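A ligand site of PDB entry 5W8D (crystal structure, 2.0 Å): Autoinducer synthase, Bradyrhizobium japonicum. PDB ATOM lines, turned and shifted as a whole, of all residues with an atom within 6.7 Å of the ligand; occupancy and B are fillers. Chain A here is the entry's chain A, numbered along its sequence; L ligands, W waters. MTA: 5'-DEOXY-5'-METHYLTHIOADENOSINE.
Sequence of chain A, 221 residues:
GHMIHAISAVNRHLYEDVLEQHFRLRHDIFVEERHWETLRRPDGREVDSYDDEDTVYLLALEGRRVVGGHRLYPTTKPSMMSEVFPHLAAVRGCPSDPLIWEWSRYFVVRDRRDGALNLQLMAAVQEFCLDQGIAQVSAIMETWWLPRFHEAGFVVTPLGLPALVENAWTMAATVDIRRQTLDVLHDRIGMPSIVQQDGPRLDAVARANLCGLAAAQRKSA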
ATOM      1  N   HIS A  35      13.894 -20.446  10.267  1.00  0.00           N
ATOM      2  CA  HIS A  35      13.018 -21.142  11.226  1.00  0.00           C
ATOM      3  C   HIS A  35      12.023 -22.094  10.553  1.00  0.00           C
ATOM      4  O   HIS A  35      10.885 -22.230  11.015  1.00  0.00           O
ATOM      5  CB  HIS A  35      12.265 -20.139  12.124  1.00  0.00           C
ATOM      6  CG  HIS A  35      13.149 -19.085  12.737  1.00  0.00           C
ATOM      7  ND1 HIS A  35      14.292 -19.384  13.445  1.00  0.00           N
ATOM      8  CD2 HIS A  35      13.032 -17.741  12.751  1.00  0.00           C
ATOM      9  CE1 HIS A  35      14.857 -18.269  13.855  1.00  0.00           C
ATOM     10  NE2 HIS A  35      14.114 -17.249  13.459  1.00  0.00           N
ATOM     11  N   TRP A  36      12.445 -22.758   9.478  1.00  0.00           N
ATOM     12  CA  TRP A  36      11.609 -23.785   8.863  1.00  0.00           C
ATOM     13  C   TRP A  36      11.815 -25.053   9.692  1.00  0.00           C
ATOM     14  O   TRP A  36      12.511 -25.992   9.281  1.00  0.00           O
ATOM     15  CB  TRP A  36      11.997 -24.006   7.398  1.00  0.00           C
ATOM     16  CG  TRP A  36      11.654 -22.864   6.467  1.00  0.00           C
ATOM     17  CD1 TRP A  36      11.170 -21.634   6.802  1.00  0.00           C
ATOM     18  CD2 TRP A  36      11.813 -22.846   5.041  1.00  0.00           C
ATOM     19  NE1 TRP A  36      11.006 -20.851   5.678  1.00  0.00           N
ATOM     20  CE2 TRP A  36      11.393 -21.573   4.582  1.00  0.00           C
ATOM     21  CE3 TRP A  36      12.270 -23.790   4.099  1.00  0.00           C
ATOM     22  CZ2 TRP A  36      11.409 -21.212   3.225  1.00  0.00           C
ATOM     23  CZ3 TRP A  36      12.282 -23.424   2.755  1.00  0.00           C
ATOM     24  CH2 TRP A  36      11.863 -22.153   2.328  1.00  0.00           C
ATOM     25  N   GLU A  37      11.183 -25.074  10.871  1.00  0.00           N
ATOM     26  CA  GLU A  37      11.414 -26.098  11.894  1.00  0.00           C
ATOM     27  C   GLU A  37      11.094 -27.532  11.488  1.00  0.00           C
ATOM     28  O   GLU A  37      11.688 -28.464  12.022  1.00  0.00           O
ATOM     29  CB  GLU A  37      10.662 -25.745  13.193  1.00  0.00           C
ATOM     30  CG  GLU A  37      11.216 -24.529  13.927  1.00  0.00           C
ATOM     31  CD  GLU A  37      12.663 -24.708  14.384  1.00  0.00           C
ATOM     32  OE1 GLU A  37      13.049 -25.828  14.775  1.00  0.00           O
ATOM     33  OE2 GLU A  37      13.411 -23.714  14.355  1.00  0.00           O
ATOM     34  N   THR A  38      10.170 -27.716  10.536  1.00  0.00           N
ATOM     35  CA  THR A  38       9.861 -29.075  10.066  1.00  0.00           C
ATOM     36  C   THR A  38      11.092 -29.750   9.454  1.00  0.00           C
ATOM     37  O   THR A  38      11.123 -30.971   9.350  1.00  0.00           O
ATOM     38  CB  THR A  38       8.690 -29.123   9.059  1.00  0.00           C
ATOM     39  OG1 THR A  38       9.113 -28.563   7.806  1.00  0.00           O
ATOM     40  CG2 THR A  38       7.460 -28.386   9.577  1.00  0.00           C
ATOM     41  N   LEU A  39      12.093 -28.955   9.063  1.00  0.00           N
ATOM     42  CA  LEU A  39      13.298 -29.469   8.422  1.00  0.00           C
ATOM     43  C   LEU A  39      14.494 -29.671   9.373  1.00  0.00           C
ATOM     44  O   LEU A  39      15.566 -30.108   8.935  1.00  0.00           O
ATOM     45  CB  LEU A  39      13.701 -28.564   7.247  1.00  0.00           C
ATOM     46  CG  LEU A  39      12.659 -28.353   6.148  1.00  0.00           C
ATOM     47  CD1 LEU A  39      13.133 -27.283   5.173  1.00  0.00           C
ATOM     48  CD2 LEU A  39      12.354 -29.662   5.423  1.00  0.00           C
ATOM     49  N   GLU A  46      20.626 -30.581   6.518  1.00  0.00           N
ATOM     50  CA  GLU A  46      19.273 -30.348   6.057  1.00  0.00           C
ATOM     51  C   GLU A  46      19.039 -31.148   4.778  1.00  0.00           C
ATOM     52  O   GLU A  46      19.440 -30.739   3.685  1.00  0.00           O
ATOM     53  CB  GLU A  46      19.023 -28.842   5.846  1.00  0.00           C
ATOM     54  CG  GLU A  46      17.547 -28.461   5.779  1.00  0.00           C
ATOM     55  CD  GLU A  46      16.932 -28.780   4.437  1.00  0.00           C
ATOM     56  OE1 GLU A  46      17.271 -28.093   3.440  1.00  0.00           O
ATOM     57  OE2 GLU A  46      16.115 -29.722   4.366  1.00  0.00           O
ATOM     58  N   ASP A  48      16.114 -33.765   2.824  1.00  0.00           N
ATOM     59  CA  ASP A  48      14.727 -34.222   2.807  1.00  0.00           C
ATOM     60  C   ASP A  48      14.548 -35.373   1.797  1.00  0.00           C
ATOM     61  O   ASP A  48      15.525 -35.890   1.261  1.00  0.00           O
ATOM     62  CB  ASP A  48      13.747 -33.042   2.579  1.00  0.00           C
ATOM     63  CG  ASP A  48      13.788 -32.467   1.159  1.00  0.00           C
ATOM     64  OD1 ASP A  48      14.423 -33.071   0.270  1.00  0.00           O
ATOM     65  OD2 ASP A  48      13.166 -31.392   0.942  1.00  0.00           O
ATOM     66  N   SER A  49      13.291 -35.763   1.553  1.00  0.00           N
ATOM     67  CA  SER A  49      12.970 -36.883   0.657  1.00  0.00           C
ATOM     68  C   SER A  49      13.325 -36.640  -0.810  1.00  0.00           C
ATOM     69  O   SER A  49      13.285 -37.566  -1.603  1.00  0.00           O
ATOM     70  CB  SER A  49      11.466 -37.200   0.730  1.00  0.00           C
ATOM     71  OG  SER A  49      11.100 -37.553   2.044  1.00  0.00           O
ATOM     72  N   TYR A  50      13.652 -35.399  -1.161  1.00  0.00           N
ATOM     73  CA  TYR A  50      13.956 -35.042  -2.561  1.00  0.00           C
ATOM     74  C   TYR A  50      15.448 -34.810  -2.765  1.00  0.00           C
ATOM     75  O   TYR A  50      15.873 -34.283  -3.799  1.00  0.00           O
ATOM     76  CB  TYR A  50      13.083 -33.853  -3.001  1.00  0.00           C
ATOM     77  CG  TYR A  50      11.667 -34.065  -2.542  1.00  0.00           C
ATOM     78  CD1 TYR A  50      10.866 -35.034  -3.135  1.00  0.00           C
ATOM     79  CD2 TYR A  50      11.158 -33.374  -1.436  1.00  0.00           C
ATOM     80  CE1 TYR A  50       9.576 -35.277  -2.691  1.00  0.00           C
ATOM     81  CE2 TYR A  50       9.864 -33.613  -0.980  1.00  0.00           C
ATOM     82  CZ  TYR A  50       9.089 -34.557  -1.613  1.00  0.00           C
ATOM     83  OH  TYR A  50       7.822 -34.805  -1.168  1.00  0.00           O
ATOM     84  N   ARG A  71      18.333 -26.369  -6.118  1.00  0.00           N
ATOM     85  CA  ARG A  71      18.264 -27.747  -6.602  1.00  0.00           C
ATOM     86  C   ARG A  71      17.068 -28.003  -7.509  1.00  0.00           C
ATOM     87  O   ARG A  71      16.057 -27.302  -7.473  1.00  0.00           O
ATOM     88  CB  ARG A  71      18.271 -28.747  -5.427  1.00  0.00           C
ATOM     89  CG  ARG A  71      17.044 -28.659  -4.563  1.00  0.00           C
ATOM     90  CD  ARG A  71      16.909 -29.810  -3.569  1.00  0.00           C
ATOM     91  NE  ARG A  71      15.603 -29.708  -2.935  1.00  0.00           N
ATOM     92  CZ  ARG A  71      15.155 -30.500  -1.961  1.00  0.00           C
ATOM     93  NH1 ARG A  71      15.907 -31.475  -1.476  1.00  0.00           N
ATOM     94  NH2 ARG A  71      13.928 -30.290  -1.475  1.00  0.00           N
ATOM     95  N   MET A  80       7.772 -32.585  -4.081  1.00  0.00           N
ATOM     96  CA  MET A  80       7.272 -31.775  -2.985  1.00  0.00           C
ATOM     97  C   MET A  80       5.866 -31.272  -3.295  1.00  0.00           C
ATOM     98  O   MET A  80       4.987 -31.290  -2.424  1.00  0.00           O
ATOM     99  CB  MET A  80       8.216 -30.601  -2.697  1.00  0.00           C
ATOM    100  CG  MET A  80       8.017 -29.968  -1.321  1.00  0.00           C
ATOM    101  SD  MET A  80       8.877 -28.392  -1.116  1.00  0.00           S
ATOM    102  CE  MET A  80      10.530 -28.821  -1.645  1.00  0.00           C
ATOM    103  N   VAL A  84       3.448 -32.920  -0.803  1.00  0.00           N
ATOM    104  CA  VAL A  84       3.304 -32.020   0.349  1.00  0.00           C
ATOM    105  C   VAL A  84       2.286 -30.918   0.090  1.00  0.00           C
ATOM    106  O   VAL A  84       1.507 -30.570   0.970  1.00  0.00           O
ATOM    107  CB  VAL A  84       4.655 -31.406   0.779  1.00  0.00           C
ATOM    108  CG1 VAL A  84       4.522 -30.694   2.124  1.00  0.00           C
ATOM    109  CG2 VAL A  84       5.721 -32.483   0.878  1.00  0.00           C
ATOM    110  N   PHE A  85       2.281 -30.373  -1.129  1.00  0.00           N
ATOM    111  CA  PHE A  85       1.464 -29.198  -1.410  1.00  0.00           C
ATOM    112  C   PHE A  85       0.509 -29.338  -2.603  1.00  0.00           C
ATOM    113  O   PHE A  85       0.329 -28.356  -3.347  1.00  0.00           O
ATOM    114  CB  PHE A  85       2.381 -27.983  -1.654  1.00  0.00           C
ATOM    115  CG  PHE A  85       3.282 -27.642  -0.499  1.00  0.00           C
ATOM    116  CD1 PHE A  85       2.762 -27.051   0.648  1.00  0.00           C
ATOM    117  CD2 PHE A  85       4.658 -27.857  -0.584  1.00  0.00           C
ATOM    118  CE1 PHE A  85       3.595 -26.716   1.710  1.00  0.00           C
ATOM    119  CE2 PHE A  85       5.491 -27.505   0.464  1.00  0.00           C
ATOM    120  CZ  PHE A  85       4.963 -26.942   1.619  1.00  0.00           C
ATOM    121  N   SER A 104      13.849 -25.851  -6.050  1.00  0.00           N
ATOM    122  CA  SER A 104      13.713 -25.535  -4.621  1.00  0.00           C
ATOM    123  C   SER A 104      15.046 -25.210  -3.972  1.00  0.00           C
ATOM    124  O   SER A 104      16.109 -25.294  -4.616  1.00  0.00           O
ATOM    125  CB  SER A 104      13.043 -26.701  -3.869  1.00  0.00           C
ATOM    126  OG  SER A 104      13.842 -27.871  -3.968  1.00  0.00           O
ATOM    127  N   ARG A 105      14.968 -24.822  -2.701  1.00  0.00           N
ATOM    128  CA  ARG A 105      16.127 -24.599  -1.826  1.00  0.00           C
ATOM    129  C   ARG A 105      17.082 -23.506  -2.321  1.00  0.00           C
ATOM    130  O   ARG A 105      18.309 -23.639  -2.225  1.00  0.00           O
ATOM    131  CB  ARG A 105      16.869 -25.920  -1.548  1.00  0.00           C
ATOM    132  CG  ARG A 105      16.060 -26.935  -0.748  1.00  0.00           C
ATOM    133  CD  ARG A 105      15.662 -26.413   0.633  1.00  0.00           C
ATOM    134  NE  ARG A 105      15.352 -27.526   1.536  1.00  0.00           N
ATOM    135  CZ  ARG A 105      14.208 -28.197   1.571  1.00  0.00           C
ATOM    136  NH1 ARG A 105      13.208 -27.884   0.749  1.00  0.00           N
ATOM    137  NH2 ARG A 105      14.059 -29.202   2.418  1.00  0.00           N
ATOM    138  N   ILE A 140       7.186 -24.284  -5.475  1.00  0.00           N
ATOM    139  CA  ILE A 140       6.323 -23.828  -4.403  1.00  0.00           C
ATOM    140  C   ILE A 140       7.080 -22.648  -3.808  1.00  0.00           C
ATOM    141  O   ILE A 140       8.218 -22.795  -3.365  1.00  0.00           O
ATOM    142  CB  ILE A 140       6.060 -24.915  -3.334  1.00  0.00           C
ATOM    143  CG1 ILE A 140       5.337 -26.118  -3.956  1.00  0.00           C
ATOM    144  CG2 ILE A 140       5.250 -24.365  -2.176  1.00  0.00           C
ATOM    145  CD1 ILE A 140       6.260 -27.280  -4.254  1.00  0.00           C
ATOM    146  N   MET A 141       6.466 -21.478  -3.813  1.00  0.00           N
ATOM    147  CA  MET A 141       7.177 -20.279  -3.384  1.00  0.00           C
ATOM    148  C   MET A 141       6.312 -19.314  -2.588  1.00  0.00           C
ATOM    149  O   MET A 141       5.098 -19.213  -2.786  1.00  0.00           O
ATOM    150  CB  MET A 141       7.703 -19.537  -4.614  1.00  0.00           C
ATOM    151  CG  MET A 141       6.602 -18.949  -5.470  1.00  0.00           C
ATOM    152  SD  MET A 141       7.099 -18.775  -7.180  1.00  0.00           S
ATOM    153  CE  MET A 141       5.827 -17.664  -7.766  1.00  0.00           C
ATOM    154  N   GLU A 142       6.953 -18.584  -1.676  1.00  0.00           N
ATOM    155  CA  GLU A 142       6.291 -17.502  -0.982  1.00  0.00           C
ATOM    156  C   GLU A 142       6.002 -16.407  -2.004  1.00  0.00           C
ATOM    157  O   GLU A 142       6.767 -16.202  -2.953  1.00  0.00           O
ATOM    158  CB  GLU A 142       7.131 -16.998   0.194  1.00  0.00           C
ATOM    159  CG  GLU A 142       7.354 -18.071   1.249  1.00  0.00           C
ATOM    160  CD  GLU A 142       7.688 -17.502   2.616  1.00  0.00           C
ATOM    161  OE1 GLU A 142       7.526 -16.284   2.820  1.00  0.00           O
ATOM    162  OE2 GLU A 142       8.122 -18.298   3.488  1.00  0.00           O
ATOM    163  N   VAL A 165       0.793 -21.039   4.183  1.00  0.00           N
ATOM    164  CA  VAL A 165       1.556 -22.222   4.552  1.00  0.00           C
ATOM    165  C   VAL A 165       2.346 -21.787   5.776  1.00  0.00           C
ATOM    166  O   VAL A 165       3.224 -20.928   5.684  1.00  0.00           O
ATOM    167  CB  VAL A 165       2.476 -22.726   3.421  1.00  0.00           C
ATOM    168  CG1 VAL A 165       3.485 -23.755   3.935  1.00  0.00           C
ATOM    169  CG2 VAL A 165       1.634 -23.329   2.289  1.00  0.00           C
ATOM    170  N   GLU A 166       2.002 -22.377   6.916  1.00  0.00           N
ATOM    171  CA  GLU A 166       2.347 -21.833   8.218  1.00  0.00           C
ATOM    172  C   GLU A 166       1.747 -20.427   8.336  1.00  0.00           C
ATOM    173  O   GLU A 166       0.534 -20.276   8.374  1.00  0.00           O
ATOM    174  CB  GLU A 166       3.868 -21.828   8.449  1.00  0.00           C
ATOM    175  CG  GLU A 166       4.500 -23.217   8.478  1.00  0.00           C
ATOM    176  CD  GLU A 166       3.959 -24.097   9.596  1.00  0.00           C
ATOM    177  OE1 GLU A 166       3.677 -23.583  10.702  1.00  0.00           O
ATOM    178  OE2 GLU A 166       3.831 -25.321   9.375  1.00  0.00           O
ATOM    179  N   THR A 170       1.772 -18.419   0.244  1.00  0.00           N
ATOM    180  CA  THR A 170       2.551 -19.312  -0.600  1.00  0.00           C
ATOM    181  C   THR A 170       1.717 -19.695  -1.818  1.00  0.00           C
ATOM    182  O   THR A 170       0.480 -19.707  -1.760  1.00  0.00           O
ATOM    183  CB  THR A 170       2.955 -20.560   0.225  1.00  0.00           C
ATOM    184  OG1 THR A 170       3.605 -20.139   1.431  1.00  0.00           O
ATOM    185  CG2 THR A 170       3.895 -21.484  -0.527  1.00  0.00           C
HETATM  186  CS  MTA L   1       8.606 -24.371  -0.086  1.00  0.00           C
HETATM  187  S5' MTA L   1       7.741 -23.060   0.714  1.00  0.00           S
HETATM  188  C5' MTA L   1       8.451 -23.139   2.332  1.00  0.00           C
HETATM  189  C4' MTA L   1       7.694 -24.094   3.247  1.00  0.00           C
HETATM  190  O4' MTA L   1       7.768 -25.433   2.749  1.00  0.00           O
HETATM  191  C2' MTA L   1       9.046 -25.434   4.754  1.00  0.00           C
HETATM  192  O2' MTA L   1       8.995 -25.954   6.088  1.00  0.00           O
HETATM  193  C3' MTA L   1       8.323 -24.106   4.638  1.00  0.00           C
HETATM  194  O3' MTA L   1       7.265 -24.038   5.599  1.00  0.00           O
HETATM  195  C1' MTA L   1       8.249 -26.303   3.785  1.00  0.00           C
HETATM  196  N9  MTA L   1       9.049 -27.402   3.184  1.00  0.00           N
HETATM  197  C8  MTA L   1      10.149 -27.311   2.416  1.00  0.00           C
HETATM  198  N7  MTA L   1      10.588 -28.543   2.050  1.00  0.00           N
HETATM  199  C5  MTA L   1       9.747 -29.441   2.598  1.00  0.00           C
HETATM  200  C6  MTA L   1       9.615 -30.920   2.637  1.00  0.00           C
HETATM  201  N6  MTA L   1      10.490 -31.733   2.003  1.00  0.00           N
HETATM  202  N1  MTA L   1       8.577 -31.442   3.349  1.00  0.00           N
HETATM  203  C2  MTA L   1       7.685 -30.676   4.003  1.00  0.00           C
HETATM  204  N3  MTA L   1       7.751 -29.339   4.010  1.00  0.00           N
HETATM  205  C4  MTA L   1       8.737 -28.686   3.350  1.00  0.00           C
HETATM  206  O   HOH W   1      10.446 -24.543  -2.738  1.00  0.00           O
HETATM  207  O   HOH W   2       7.604 -34.001   3.639  1.00  0.00           O
HETATM  208  O   HOH W   3       5.430 -28.470   5.446  1.00  0.00           O
HETATM  209  O   HOH W   4      10.676 -34.516   2.637  1.00  0.00           O
HETATM  210  O   HOH W   5       5.955 -21.470   5.359  1.00  0.00           O
HETATM  211  O   HOH W   6       8.235 -25.454   9.104  1.00  0.00           O
HETATM  212  O   HOH W   7       5.938 -20.843   2.671  1.00  0.00           O
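The side-chain hydroxyl (OG1) of Thr 38 is in hydrogen-bond range of an oxygen (O2') of the ligand, at 3.1 Å. A nitrogen (N7) of the ligand lies within hydrogen-bond range of the guanidinium group (NH1) of Arg 105 (3.0 Å). The side-chain carboxylate (OD2) of Asp 48 sits at hydrogen-bond distance from a nitrogen (N6) of the ligand.
The side-chain carboxylate of Asp 48 is in salt-bridge range of the guanidinium group of Arg 105, 2.8 Å away. The backbone NH of Tyr 50 sits at hydrogen-bond distance from the side-chain carboxylate of Asp 48 (2.8 Å). NH2 of Arg 71 lies within salt-bridge range of OD2 of Asp 48 (2.8 Å). The backbone NH (N) of Phe 85 is in hydrogen-bond range of the backbone carbonyl oxygen (O) of Met 80. The guanidinium group (NE) of Arg 105 lies within salt-bridge range of the side-chain carboxylate (OE1) of Glu 46 (2.8 Å).
SD of Met 80 lies close to N7 of the ligand (3.6 Å). Trp 36 touches the ligand. Leu 39 touches the ligand. Tyr 50 touches the ligand. Val 84 touches the ligand. Phe 85 touches the ligand. Ile 140 touches the ligand (O to CS, 3.7 Å). Hydrophobic or aromatic side chains that line the ligand: Trp 36, Leu 39, Tyr 50, Met 80, Val 84, Phe 85 and Ile 140. Of the 21 residues printed, 10 come within 4 Å of the ligand. The nearest printed residue that does not touch the ligand is Glu 166 (4.1 Å).
Water W4 lies within hydrogen-bond range of a nitrogen (N6) of the ligand (2.9 Å) and the backbone NH (N) of Ser 49 (3.1 Å). Water W5 lies within hydrogen-bond range of the backbone carbonyl oxygen (O) of Val 165 (2.8 Å) and an oxygen (O3') of the ligand (2.9 Å). Water W6 lies within hydrogen-bond range of O2' of the ligand (3.2 Å), N of Thr 38 (3.3 Å) and N of Glu 37 (3.5 Å). Water W7 lies within hydrogen-bond range of OG1 of Thr 170, OE2 of Glu 142 and S5' of the ligand.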
